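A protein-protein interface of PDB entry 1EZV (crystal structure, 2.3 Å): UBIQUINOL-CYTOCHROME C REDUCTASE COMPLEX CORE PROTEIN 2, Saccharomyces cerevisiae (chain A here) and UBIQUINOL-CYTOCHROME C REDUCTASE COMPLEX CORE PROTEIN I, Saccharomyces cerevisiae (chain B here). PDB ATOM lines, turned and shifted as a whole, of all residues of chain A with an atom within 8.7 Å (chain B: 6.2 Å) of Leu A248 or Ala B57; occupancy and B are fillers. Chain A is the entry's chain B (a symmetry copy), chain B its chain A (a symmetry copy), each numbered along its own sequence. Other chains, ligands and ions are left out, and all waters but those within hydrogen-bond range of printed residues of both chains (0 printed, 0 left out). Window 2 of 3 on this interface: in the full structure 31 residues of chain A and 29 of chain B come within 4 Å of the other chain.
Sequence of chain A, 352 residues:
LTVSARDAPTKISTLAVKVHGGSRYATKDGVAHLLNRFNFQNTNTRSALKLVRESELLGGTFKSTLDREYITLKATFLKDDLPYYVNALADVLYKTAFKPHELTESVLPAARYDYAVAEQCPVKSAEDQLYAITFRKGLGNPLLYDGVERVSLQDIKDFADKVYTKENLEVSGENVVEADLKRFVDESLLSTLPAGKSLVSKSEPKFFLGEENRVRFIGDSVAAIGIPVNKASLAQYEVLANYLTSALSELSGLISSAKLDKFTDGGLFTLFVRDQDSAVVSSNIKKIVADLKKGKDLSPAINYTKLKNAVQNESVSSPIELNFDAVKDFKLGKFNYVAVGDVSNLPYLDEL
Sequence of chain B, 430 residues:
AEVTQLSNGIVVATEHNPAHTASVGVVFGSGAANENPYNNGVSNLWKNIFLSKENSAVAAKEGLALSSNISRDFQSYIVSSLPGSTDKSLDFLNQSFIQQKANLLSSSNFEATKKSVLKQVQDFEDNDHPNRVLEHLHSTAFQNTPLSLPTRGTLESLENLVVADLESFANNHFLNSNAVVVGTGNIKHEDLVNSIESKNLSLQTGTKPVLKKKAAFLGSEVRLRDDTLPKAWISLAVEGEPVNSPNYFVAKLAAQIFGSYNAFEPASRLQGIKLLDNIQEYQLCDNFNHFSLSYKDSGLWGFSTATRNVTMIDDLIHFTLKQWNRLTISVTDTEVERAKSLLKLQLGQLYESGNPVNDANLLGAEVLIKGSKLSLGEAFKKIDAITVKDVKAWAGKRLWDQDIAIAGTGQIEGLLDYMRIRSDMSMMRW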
ATOM      1  N   VAL A 239      25.947  35.577 -22.941  1.00  0.00           N
ATOM      2  CA  VAL A 239      25.196  34.452 -23.497  1.00  0.00           C
ATOM      3  C   VAL A 239      25.157  33.300 -22.499  1.00  0.00           C
ATOM      4  O   VAL A 239      24.164  32.584 -22.412  1.00  0.00           O
ATOM      5  CB  VAL A 239      25.784  33.963 -24.871  1.00  0.00           C
ATOM      6  CG1 VAL A 239      26.546  35.091 -25.550  1.00  0.00           C
ATOM      7  CG2 VAL A 239      26.680  32.734 -24.695  1.00  0.00           C
ATOM      8  N   ASN A 242      22.403  34.137 -20.058  1.00  0.00           N
ATOM      9  CA  ASN A 242      21.118  33.932 -20.715  1.00  0.00           C
ATOM     10  C   ASN A 242      20.886  32.477 -21.119  1.00  0.00           C
ATOM     11  O   ASN A 242      19.753  32.074 -21.394  1.00  0.00           O
ATOM     12  CB  ASN A 242      21.008  34.832 -21.945  1.00  0.00           C
ATOM     13  CG  ASN A 242      20.321  36.142 -21.641  1.00  0.00           C
ATOM     14  OD1 ASN A 242      20.869  37.214 -21.889  1.00  0.00           O
ATOM     15  ND2 ASN A 242      19.113  36.065 -21.093  1.00  0.00           N
ATOM     16  N   TYR A 243      21.970  31.710 -21.206  1.00  0.00           N
ATOM     17  CA  TYR A 243      21.891  30.270 -21.436  1.00  0.00           C
ATOM     18  C   TYR A 243      21.437  29.587 -20.150  1.00  0.00           C
ATOM     19  O   TYR A 243      20.483  28.807 -20.160  1.00  0.00           O
ATOM     20  CB  TYR A 243      23.261  29.734 -21.886  1.00  0.00           C
ATOM     21  CG  TYR A 243      23.420  28.225 -21.862  1.00  0.00           C
ATOM     22  CD1 TYR A 243      22.734  27.409 -22.766  1.00  0.00           C
ATOM     23  CD2 TYR A 243      24.296  27.616 -20.959  1.00  0.00           C
ATOM     24  CE1 TYR A 243      22.917  26.023 -22.770  1.00  0.00           C
ATOM     25  CE2 TYR A 243      24.487  26.233 -20.954  1.00  0.00           C
ATOM     26  CZ  TYR A 243      23.794  25.443 -21.858  1.00  0.00           C
ATOM     27  OH  TYR A 243      23.963  24.077 -21.826  1.00  0.00           O
ATOM     28  N   LEU A 244      22.044  29.979 -19.031  1.00  0.00           N
ATOM     29  CA  LEU A 244      21.724  29.397 -17.731  1.00  0.00           C
ATOM     30  C   LEU A 244      20.321  29.774 -17.252  1.00  0.00           C
ATOM     31  O   LEU A 244      19.732  29.069 -16.433  1.00  0.00           O
ATOM     32  CB  LEU A 244      22.761  29.826 -16.690  1.00  0.00           C
ATOM     33  CG  LEU A 244      24.212  29.403 -16.930  1.00  0.00           C
ATOM     34  CD1 LEU A 244      25.070  29.827 -15.752  1.00  0.00           C
ATOM     35  CD2 LEU A 244      24.294  27.905 -17.130  1.00  0.00           C
ATOM     36  N   THR A 245      19.788  30.873 -17.784  1.00  0.00           N
ATOM     37  CA  THR A 245      18.435  31.326 -17.462  1.00  0.00           C
ATOM     38  C   THR A 245      17.506  31.095 -18.655  1.00  0.00           C
ATOM     39  O   THR A 245      16.794  32.001 -19.093  1.00  0.00           O
ATOM     40  CB  THR A 245      18.425  32.832 -17.086  1.00  0.00           C
ATOM     41  OG1 THR A 245      19.483  33.104 -16.158  1.00  0.00           O
ATOM     42  CG2 THR A 245      17.092  33.225 -16.446  1.00  0.00           C
ATOM     43  N   SER A 246      17.565  29.890 -19.216  1.00  0.00           N
ATOM     44  CA  SER A 246      16.703  29.520 -20.335  1.00  0.00           C
ATOM     45  C   SER A 246      16.452  28.016 -20.379  1.00  0.00           C
ATOM     46  O   SER A 246      17.143  27.241 -19.715  1.00  0.00           O
ATOM     47  CB  SER A 246      17.313  29.982 -21.662  1.00  0.00           C
ATOM     48  OG  SER A 246      18.620  29.469 -21.838  1.00  0.00           O
ATOM     49  N   ALA A 247      15.477  27.612 -21.190  1.00  0.00           N
ATOM     50  CA  ALA A 247      15.062  26.216 -21.268  1.00  0.00           C
ATOM     51  C   ALA A 247      16.047  25.351 -22.055  1.00  0.00           C
ATOM     52  O   ALA A 247      15.916  24.123 -22.095  1.00  0.00           O
ATOM     53  CB  ALA A 247      13.677  26.123 -21.879  1.00  0.00           C
ATOM     54  N   LEU A 248      17.045  25.995 -22.656  1.00  0.00           N
ATOM     55  CA  LEU A 248      18.108  25.295 -23.370  1.00  0.00           C
ATOM     56  C   LEU A 248      19.012  24.557 -22.394  1.00  0.00           C
ATOM     57  O   LEU A 248      19.330  23.384 -22.594  1.00  0.00           O
ATOM     58  CB  LEU A 248      18.931  26.288 -24.190  1.00  0.00           C
ATOM     59  CG  LEU A 248      18.141  27.112 -25.206  1.00  0.00           C
ATOM     60  CD1 LEU A 248      19.050  28.133 -25.858  1.00  0.00           C
ATOM     61  CD2 LEU A 248      17.526  26.198 -26.248  1.00  0.00           C
ATOM     62  N   SER A 249      19.386  25.235 -21.312  1.00  0.00           N
ATOM     63  CA  SER A 249      20.190  24.619 -20.266  1.00  0.00           C
ATOM     64  C   SER A 249      19.356  23.666 -19.423  1.00  0.00           C
ATOM     65  O   SER A 249      18.221  23.974 -19.055  1.00  0.00           O
ATOM     66  CB  SER A 249      20.807  25.686 -19.365  1.00  0.00           C
ATOM     67  OG  SER A 249      21.541  25.086 -18.314  1.00  0.00           O
ATOM     68  N   GLU A 250      19.926  22.500 -19.135  1.00  0.00           N
ATOM     69  CA  GLU A 250      19.270  21.511 -18.291  1.00  0.00           C
ATOM     70  C   GLU A 250      19.302  21.961 -16.837  1.00  0.00           C
ATOM     71  O   GLU A 250      18.406  21.636 -16.057  1.00  0.00           O
ATOM     72  CB  GLU A 250      19.960  20.151 -18.422  1.00  0.00           C
ATOM     73  CG  GLU A 250      19.695  19.437 -19.742  1.00  0.00           C
ATOM     74  CD  GLU A 250      19.976  17.943 -19.667  1.00  0.00           C
ATOM     75  OE1 GLU A 250      21.162  17.561 -19.541  1.00  0.00           O
ATOM     76  OE2 GLU A 250      19.009  17.151 -19.728  1.00  0.00           O
ATOM     77  N   LEU A 251      20.312  22.755 -16.496  1.00  0.00           N
ATOM     78  CA  LEU A 251      20.498  23.207 -15.124  1.00  0.00           C
ATOM     79  C   LEU A 251      19.968  24.624 -14.869  1.00  0.00           C
ATOM     80  O   LEU A 251      20.443  25.323 -13.971  1.00  0.00           O
ATOM     81  CB  LEU A 251      21.978  23.103 -14.739  1.00  0.00           C
ATOM     82  CG  LEU A 251      23.027  23.422 -15.806  1.00  0.00           C
ATOM     83  CD1 LEU A 251      23.358  24.900 -15.792  1.00  0.00           C
ATOM     84  CD2 LEU A 251      24.275  22.611 -15.534  1.00  0.00           C
ATOM     85  N   SER A 252      18.925  25.007 -15.602  1.00  0.00           N
ATOM     86  CA  SER A 252      18.271  26.293 -15.388  1.00  0.00           C
ATOM     87  C   SER A 252      17.358  26.253 -14.165  1.00  0.00           C
ATOM     88  O   SER A 252      17.268  27.226 -13.418  1.00  0.00           O
ATOM     89  CB  SER A 252      17.468  26.704 -16.629  1.00  0.00           C
ATOM     90  OG  SER A 252      16.430  25.783 -16.919  1.00  0.00           O
ATOM     91  N   LYS A 296      30.336  23.819 -21.882  1.00  0.00           N
ATOM     92  CA  LYS A 296      29.909  23.678 -23.273  1.00  0.00           C
ATOM     93  C   LYS A 296      29.172  24.935 -23.729  1.00  0.00           C
ATOM     94  O   LYS A 296      29.201  25.954 -23.039  1.00  0.00           O
ATOM     95  CB  LYS A 296      28.991  22.458 -23.427  1.00  0.00           C
ATOM     96  CG  LYS A 296      27.775  22.448 -22.502  1.00  0.00           C
ATOM     97  CD  LYS A 296      28.050  21.667 -21.224  1.00  0.00           C
ATOM     98  CE  LYS A 296      26.925  20.695 -20.911  1.00  0.00           C
ATOM     99  NZ  LYS A 296      27.349  19.677 -19.913  1.00  0.00           N
ATOM    100  N   ASP A 297      28.585  24.875 -24.926  1.00  0.00           N
ATOM    101  CA  ASP A 297      27.650  25.896 -25.407  1.00  0.00           C
ATOM    102  C   ASP A 297      27.158  25.580 -26.821  1.00  0.00           C
ATOM    103  O   ASP A 297      26.016  25.157 -27.002  1.00  0.00           O
ATOM    104  CB  ASP A 297      28.298  27.285 -25.386  1.00  0.00           C
ATOM    105  CG  ASP A 297      27.279  28.411 -25.390  1.00  0.00           C
ATOM    106  OD1 ASP A 297      27.160  29.107 -26.420  1.00  0.00           O
ATOM    107  OD2 ASP A 297      26.619  28.624 -24.352  1.00  0.00           O
ATOM    108  N   LEU A 298      28.045  25.753 -27.803  1.00  0.00           N
ATOM    109  CA  LEU A 298      27.728  25.590 -29.227  1.00  0.00           C
ATOM    110  C   LEU A 298      26.767  26.656 -29.758  1.00  0.00           C
ATOM    111  O   LEU A 298      25.993  26.401 -30.683  1.00  0.00           O
ATOM    112  CB  LEU A 298      27.164  24.189 -29.504  1.00  0.00           C
ATOM    113  CG  LEU A 298      28.181  23.058 -29.662  1.00  0.00           C
ATOM    114  CD1 LEU A 298      27.815  21.901 -28.747  1.00  0.00           C
ATOM    115  CD2 LEU A 298      28.220  22.606 -31.114  1.00  0.00           C
ATOM    116  N   SER A 299      26.854  27.856 -29.182  1.00  0.00           N
ATOM    117  CA  SER A 299      26.076  29.026 -29.606  1.00  0.00           C
ATOM    118  C   SER A 299      24.574  28.785 -29.777  1.00  0.00           C
ATOM    119  O   SER A 299      23.956  29.301 -30.711  1.00  0.00           O
ATOM    120  CB  SER A 299      26.659  29.615 -30.902  1.00  0.00           C
ATOM    121  OG  SER A 299      26.444  28.764 -32.017  1.00  0.00           O
ATOM    122  N   PRO A 300      23.951  28.070 -28.827  1.00  0.00           N
ATOM    123  CA  PRO A 300      22.551  27.683 -29.020  1.00  0.00           C
ATOM    124  C   PRO A 300      21.608  28.874 -28.845  1.00  0.00           C
ATOM    125  O   PRO A 300      20.634  29.024 -29.587  1.00  0.00           O
ATOM    126  CB  PRO A 300      22.330  26.614 -27.951  1.00  0.00           C
ATOM    127  CG  PRO A 300      23.454  26.820 -26.926  1.00  0.00           C
ATOM    128  CD  PRO A 300      24.353  27.921 -27.419  1.00  0.00           C
ATOM    129  N   ALA A 301      21.976  29.768 -27.929  1.00  0.00           N
ATOM    130  CA  ALA A 301      21.167  30.932 -27.595  1.00  0.00           C
ATOM    131  C   ALA A 301      21.603  32.174 -28.362  1.00  0.00           C
ATOM    132  O   ALA A 301      21.070  33.252 -28.136  1.00  0.00           O
ATOM    133  CB  ALA A 301      21.239  31.197 -26.093  1.00  0.00           C
ATOM    134  N   ILE A 302      22.510  32.006 -29.320  1.00  0.00           N
ATOM    135  CA  ILE A 302      23.169  33.137 -29.971  1.00  0.00           C
ATOM    136  C   ILE A 302      22.210  34.165 -30.588  1.00  0.00           C
ATOM    137  O   ILE A 302      22.555  35.341 -30.722  1.00  0.00           O
ATOM    138  CB  ILE A 302      24.199  32.637 -31.029  1.00  0.00           C
ATOM    139  CG1 ILE A 302      25.523  33.382 -30.850  1.00  0.00           C
ATOM    140  CG2 ILE A 302      23.660  32.794 -32.449  1.00  0.00           C
ATOM    141  CD1 ILE A 302      26.205  33.107 -29.518  1.00  0.00           C
ATOM    142  N   ASN A 303      20.993  33.727 -30.905  1.00  0.00           N
ATOM    143  CA  ASN A 303      19.948  34.626 -31.387  1.00  0.00           C
ATOM    144  C   ASN A 303      18.977  34.986 -30.266  1.00  0.00           C
ATOM    145  O   ASN A 303      18.339  36.039 -30.298  1.00  0.00           O
ATOM    146  CB  ASN A 303      19.184  33.979 -32.544  1.00  0.00           C
ATOM    147  CG  ASN A 303      20.067  33.710 -33.746  1.00  0.00           C
ATOM    148  OD1 ASN A 303      20.477  34.634 -34.450  1.00  0.00           O
ATOM    149  ND2 ASN A 303      20.381  32.441 -33.977  1.00  0.00           N
ATOM    150  N   TYR A 304      18.868  34.094 -29.284  1.00  0.00           N
ATOM    151  CA  TYR A 304      18.028  34.308 -28.109  1.00  0.00           C
ATOM    152  C   TYR A 304      18.691  35.248 -27.099  1.00  0.00           C
ATOM    153  O   TYR A 304      18.038  36.138 -26.559  1.00  0.00           O
ATOM    154  CB  TYR A 304      17.709  32.959 -27.452  1.00  0.00           C
ATOM    155  CG  TYR A 304      17.065  33.053 -26.083  1.00  0.00           C
ATOM    156  CD1 TYR A 304      17.809  32.813 -24.927  1.00  0.00           C
ATOM    157  CD2 TYR A 304      15.710  33.359 -25.944  1.00  0.00           C
ATOM    158  CE1 TYR A 304      17.224  32.872 -23.669  1.00  0.00           C
ATOM    159  CE2 TYR A 304      15.113  33.421 -24.686  1.00  0.00           C
ATOM    160  CZ  TYR A 304      15.877  33.175 -23.554  1.00  0.00           C
ATOM    161  OH  TYR A 304      15.296  33.223 -22.307  1.00  0.00           O
ATOM    162  N   THR A 305      19.973  35.027 -26.823  1.00  0.00           N
ATOM    163  CA  THR A 305      20.745  35.917 -25.959  1.00  0.00           C
ATOM    164  C   THR A 305      21.022  37.248 -26.656  1.00  0.00           C
ATOM    165  O   THR A 305      21.519  38.189 -26.041  1.00  0.00           O
ATOM    166  CB  THR A 305      22.085  35.272 -25.531  1.00  0.00           C
ATOM    167  OG1 THR A 305      22.760  36.135 -24.608  1.00  0.00           O
ATOM    168  CG2 THR A 305      22.981  35.042 -26.729  1.00  0.00           C
ATOM    169  N   SER B  52       6.318  25.533 -20.521  1.00  0.00           N
ATOM    170  CA  SER B  52       7.077  24.410 -19.979  1.00  0.00           C
ATOM    171  C   SER B  52       8.443  24.277 -20.638  1.00  0.00           C
ATOM    172  O   SER B  52       8.616  24.665 -21.791  1.00  0.00           O
ATOM    173  CB  SER B  52       6.299  23.108 -20.162  1.00  0.00           C
ATOM    174  OG  SER B  52       7.049  21.999 -19.693  1.00  0.00           O
ATOM    175  N   LYS B  53       9.373  23.633 -19.936  1.00  0.00           N
ATOM    176  CA  LYS B  53      10.755  23.492 -20.395  1.00  0.00           C
ATOM    177  C   LYS B  53      10.848  22.883 -21.793  1.00  0.00           C
ATOM    178  O   LYS B  53      11.708  23.267 -22.587  1.00  0.00           O
ATOM    179  CB  LYS B  53      11.559  22.644 -19.402  1.00  0.00           C
ATOM    180  CG  LYS B  53      13.042  22.521 -19.740  1.00  0.00           C
ATOM    181  CD  LYS B  53      13.812  21.756 -18.670  1.00  0.00           C
ATOM    182  CE  LYS B  53      14.180  22.656 -17.495  1.00  0.00           C
ATOM    183  NZ  LYS B  53      15.140  22.004 -16.556  1.00  0.00           N
ATOM    184  N   GLU B  54       9.917  21.984 -22.108  1.00  0.00           N
ATOM    185  CA  GLU B  54       9.865  21.347 -23.420  1.00  0.00           C
ATOM    186  C   GLU B  54       9.523  22.338 -24.527  1.00  0.00           C
ATOM    187  O   GLU B  54      10.258  22.459 -25.505  1.00  0.00           O
ATOM    188  CB  GLU B  54       8.841  20.212 -23.420  1.00  0.00           C
ATOM    189  CG  GLU B  54       9.324  18.937 -22.750  1.00  0.00           C
ATOM    190  CD  GLU B  54       8.631  17.700 -23.290  1.00  0.00           C
ATOM    191  OE1 GLU B  54       7.409  17.546 -23.060  1.00  0.00           O
ATOM    192  OE2 GLU B  54       9.306  16.891 -23.961  1.00  0.00           O
ATOM    193  N   ASN B  55       8.407  23.044 -24.370  1.00  0.00           N
ATOM    194  CA  ASN B  55       7.954  24.000 -25.373  1.00  0.00           C
ATOM    195  C   ASN B  55       8.843  25.241 -25.403  1.00  0.00           C
ATOM    196  O   ASN B  55       8.992  25.882 -26.442  1.00  0.00           O
ATOM    197  CB  ASN B  55       6.508  24.410 -25.092  1.00  0.00           C
ATOM    198  CG  ASN B  55       5.822  25.010 -26.303  1.00  0.00           C
ATOM    199  OD1 ASN B  55       5.839  24.434 -27.389  1.00  0.00           O
ATOM    200  ND2 ASN B  55       5.194  26.163 -26.116  1.00  0.00           N
ATOM    201  N   SER B  56       9.468  25.541 -24.269  1.00  0.00           N
ATOM    202  CA  SER B  56      10.246  26.766 -24.116  1.00  0.00           C
ATOM    203  C   SER B  56      11.651  26.630 -24.700  1.00  0.00           C
ATOM    204  O   SER B  56      12.273  27.628 -25.068  1.00  0.00           O
ATOM    205  CB  SER B  56      10.326  27.157 -22.635  1.00  0.00           C
ATOM    206  OG  SER B  56      10.324  28.565 -22.471  1.00  0.00           O
ATOM    207  N   ALA B  57      12.154  25.400 -24.765  1.00  0.00           N
ATOM    208  CA  ALA B  57      13.451  25.126 -25.383  1.00  0.00           C
ATOM    209  C   ALA B  57      13.351  25.131 -26.907  1.00  0.00           C
ATOM    210  O   ALA B  57      14.272  25.574 -27.596  1.00  0.00           O
ATOM    211  CB  ALA B  57      13.994  23.788 -24.896  1.00  0.00           C
ATOM    212  N   VAL B  58      12.217  24.656 -27.422  1.00  0.00           N
ATOM    213  CA  VAL B  58      11.955  24.647 -28.858  1.00  0.00           C
ATOM    214  C   VAL B  58      11.865  26.071 -29.403  1.00  0.00           C
ATOM    215  O   VAL B  58      12.235  26.325 -30.549  1.00  0.00           O
ATOM    216  CB  VAL B  58      10.642  23.881 -29.182  1.00  0.00           C
ATOM    217  CG1 VAL B  58      10.321  23.962 -30.667  1.00  0.00           C
ATOM    218  CG2 VAL B  58      10.773  22.427 -28.758  1.00  0.00           C
ATOM    219  N   ALA B  59      11.442  27.005 -28.554  1.00  0.00           N
ATOM    220  CA  ALA B  59      11.362  28.414 -28.931  1.00  0.00           C
ATOM    221  C   ALA B  59      12.700  29.137 -28.773  1.00  0.00           C
ATOM    222  O   ALA B  59      13.004  30.055 -29.532  1.00  0.00           O
ATOM    223  CB  ALA B  59      10.290  29.116 -28.111  1.00  0.00           C
ATOM    224  N   ALA B  60      13.495  28.714 -27.793  1.00  0.00           N
ATOM    225  CA  ALA B  60      14.768  29.364 -27.494  1.00  0.00           C
ATOM    226  C   ALA B  60      15.867  28.975 -28.480  1.00  0.00           C
ATOM    227  O   ALA B  60      16.834  29.718 -28.663  1.00  0.00           O
ATOM    228  CB  ALA B  60      15.197  29.040 -26.075  1.00  0.00           C
ATOM    229  N   LYS B  61      15.730  27.798 -29.090  1.00  0.00           N
ATOM    230  CA  LYS B  61      16.591  27.398 -30.203  1.00  0.00           C
ATOM    231  C   LYS B  61      16.404  28.374 -31.361  1.00  0.00           C
ATOM    232  O   LYS B  61      17.373  28.925 -31.887  1.00  0.00           O
ATOM    233  CB  LYS B  61      16.236  25.981 -30.676  1.00  0.00           C
ATOM    234  CG  LYS B  61      16.603  24.862 -29.709  1.00  0.00           C
ATOM    235  CD  LYS B  61      18.089  24.521 -29.766  1.00  0.00           C
ATOM    236  CE  LYS B  61      18.405  23.296 -28.915  1.00  0.00           C
ATOM    237  NZ  LYS B  61      19.869  23.027 -28.836  1.00  0.00           N
ATOM    238  N   GLU B  62      15.141  28.650 -31.677  1.00  0.00           N
ATOM    239  CA  GLU B  62      14.769  29.535 -32.775  1.00  0.00           C
ATOM    240  C   GLU B  62      15.004  31.010 -32.432  1.00  0.00           C
ATOM    241  O   GLU B  62      14.845  31.886 -33.287  1.00  0.00           O
ATOM    242  CB  GLU B  62      13.297  29.311 -33.141  1.00  0.00           C
ATOM    243  CG  GLU B  62      12.946  29.622 -34.592  1.00  0.00           C
ATOM    244  CD  GLU B  62      13.412  28.545 -35.556  1.00  0.00           C
ATOM    245  OE1 GLU B  62      12.709  27.520 -35.685  1.00  0.00           O
ATOM    246  OE2 GLU B  62      14.468  28.730 -36.199  1.00  0.00           O
ATOM    247  N   LEU B  66       8.966  33.465 -24.791  1.00  0.00           N
ATOM    248  CA  LEU B  66       7.573  33.127 -24.510  1.00  0.00           C
ATOM    249  C   LEU B  66       6.987  33.890 -23.324  1.00  0.00           C
ATOM    250  O   LEU B  66       7.650  34.077 -22.301  1.00  0.00           O
ATOM    251  CB  LEU B  66       7.439  31.623 -24.267  1.00  0.00           C
ATOM    252  CG  LEU B  66       7.717  30.708 -25.462  1.00  0.00           C
ATOM    253  CD1 LEU B  66       7.609  29.258 -25.028  1.00  0.00           C
ATOM    254  CD2 LEU B  66       6.736  31.009 -26.578  1.00  0.00           C
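Lys B53 touches Ala A247.
Ala A247 touches Ser B56 (CB to C, 3.5 Å).
Ala A247 touches Ala B57.
CD2 of Leu A248 touches O of Ala B57, at 3.6 Å.
CG of Leu A248 touches CB of Ala B60, 3.6 Å away.
Leu A248 touches Lys B61.
CE of Lys B53 touches OG of Ser A252 (3.9 Å).
Ala B60 touches Pro A300 (O to O, 3.97 Å).
Lys B61 touches Pro A300.
Tyr A304 touches Ala B60.
Hydrophobic or aromatic side chains of chain A that line the printed part of chain B: Ala A247, Leu A248 and Tyr A304.
Among the printed residues, no Asp or Glu carboxylate lies within 4 Å of a Lys or Arg side-chain nitrogen of the other chain.
Leu A248 touches just these residues of chain B: Ala B57, Ala B60 and Lys B61.
Of chain A, only Ala A247 (3.3 Å) and Leu A248 (3.6 Å) come within 4 Å of Ala B57.
Ser B56 touches just one residue of chain A: Ala A247 (3.5 Å).
Ala B60 touches just these residues of chain A: Leu A248, Pro A300 and Tyr A304.
Of the printed residues of chain B, Ala A247 touches Lys B53, Ser B56 and Ala B57.
Printed residues of chain B within 4 Å of Pro A300: Ala B60 (3.97 Å) and Lys B61 (3.99 Å).
Printed residues of chain B within 4 Å of Tyr A304: Ala B60.
Asn B55 touches none of the printed residues of chain A.
The nearest residue of chain A that does not touch Ala B57 is Ser A246 (6.5 Å).
The backbone carbonyl oxygen (O) of Ser A249 sits at hydrogen-bond distance from the side-chain hydroxyl (OG) of Ser A252 (3.3 Å).
OG of Ser A252 sits close to O of Ser A246 (3.2 Å).
The backbone carbonyl oxygen (O) of Glu A250 sits at hydrogen-bond distance from the side-chain amino group (NZ) of Lys B53 (3.3 Å).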
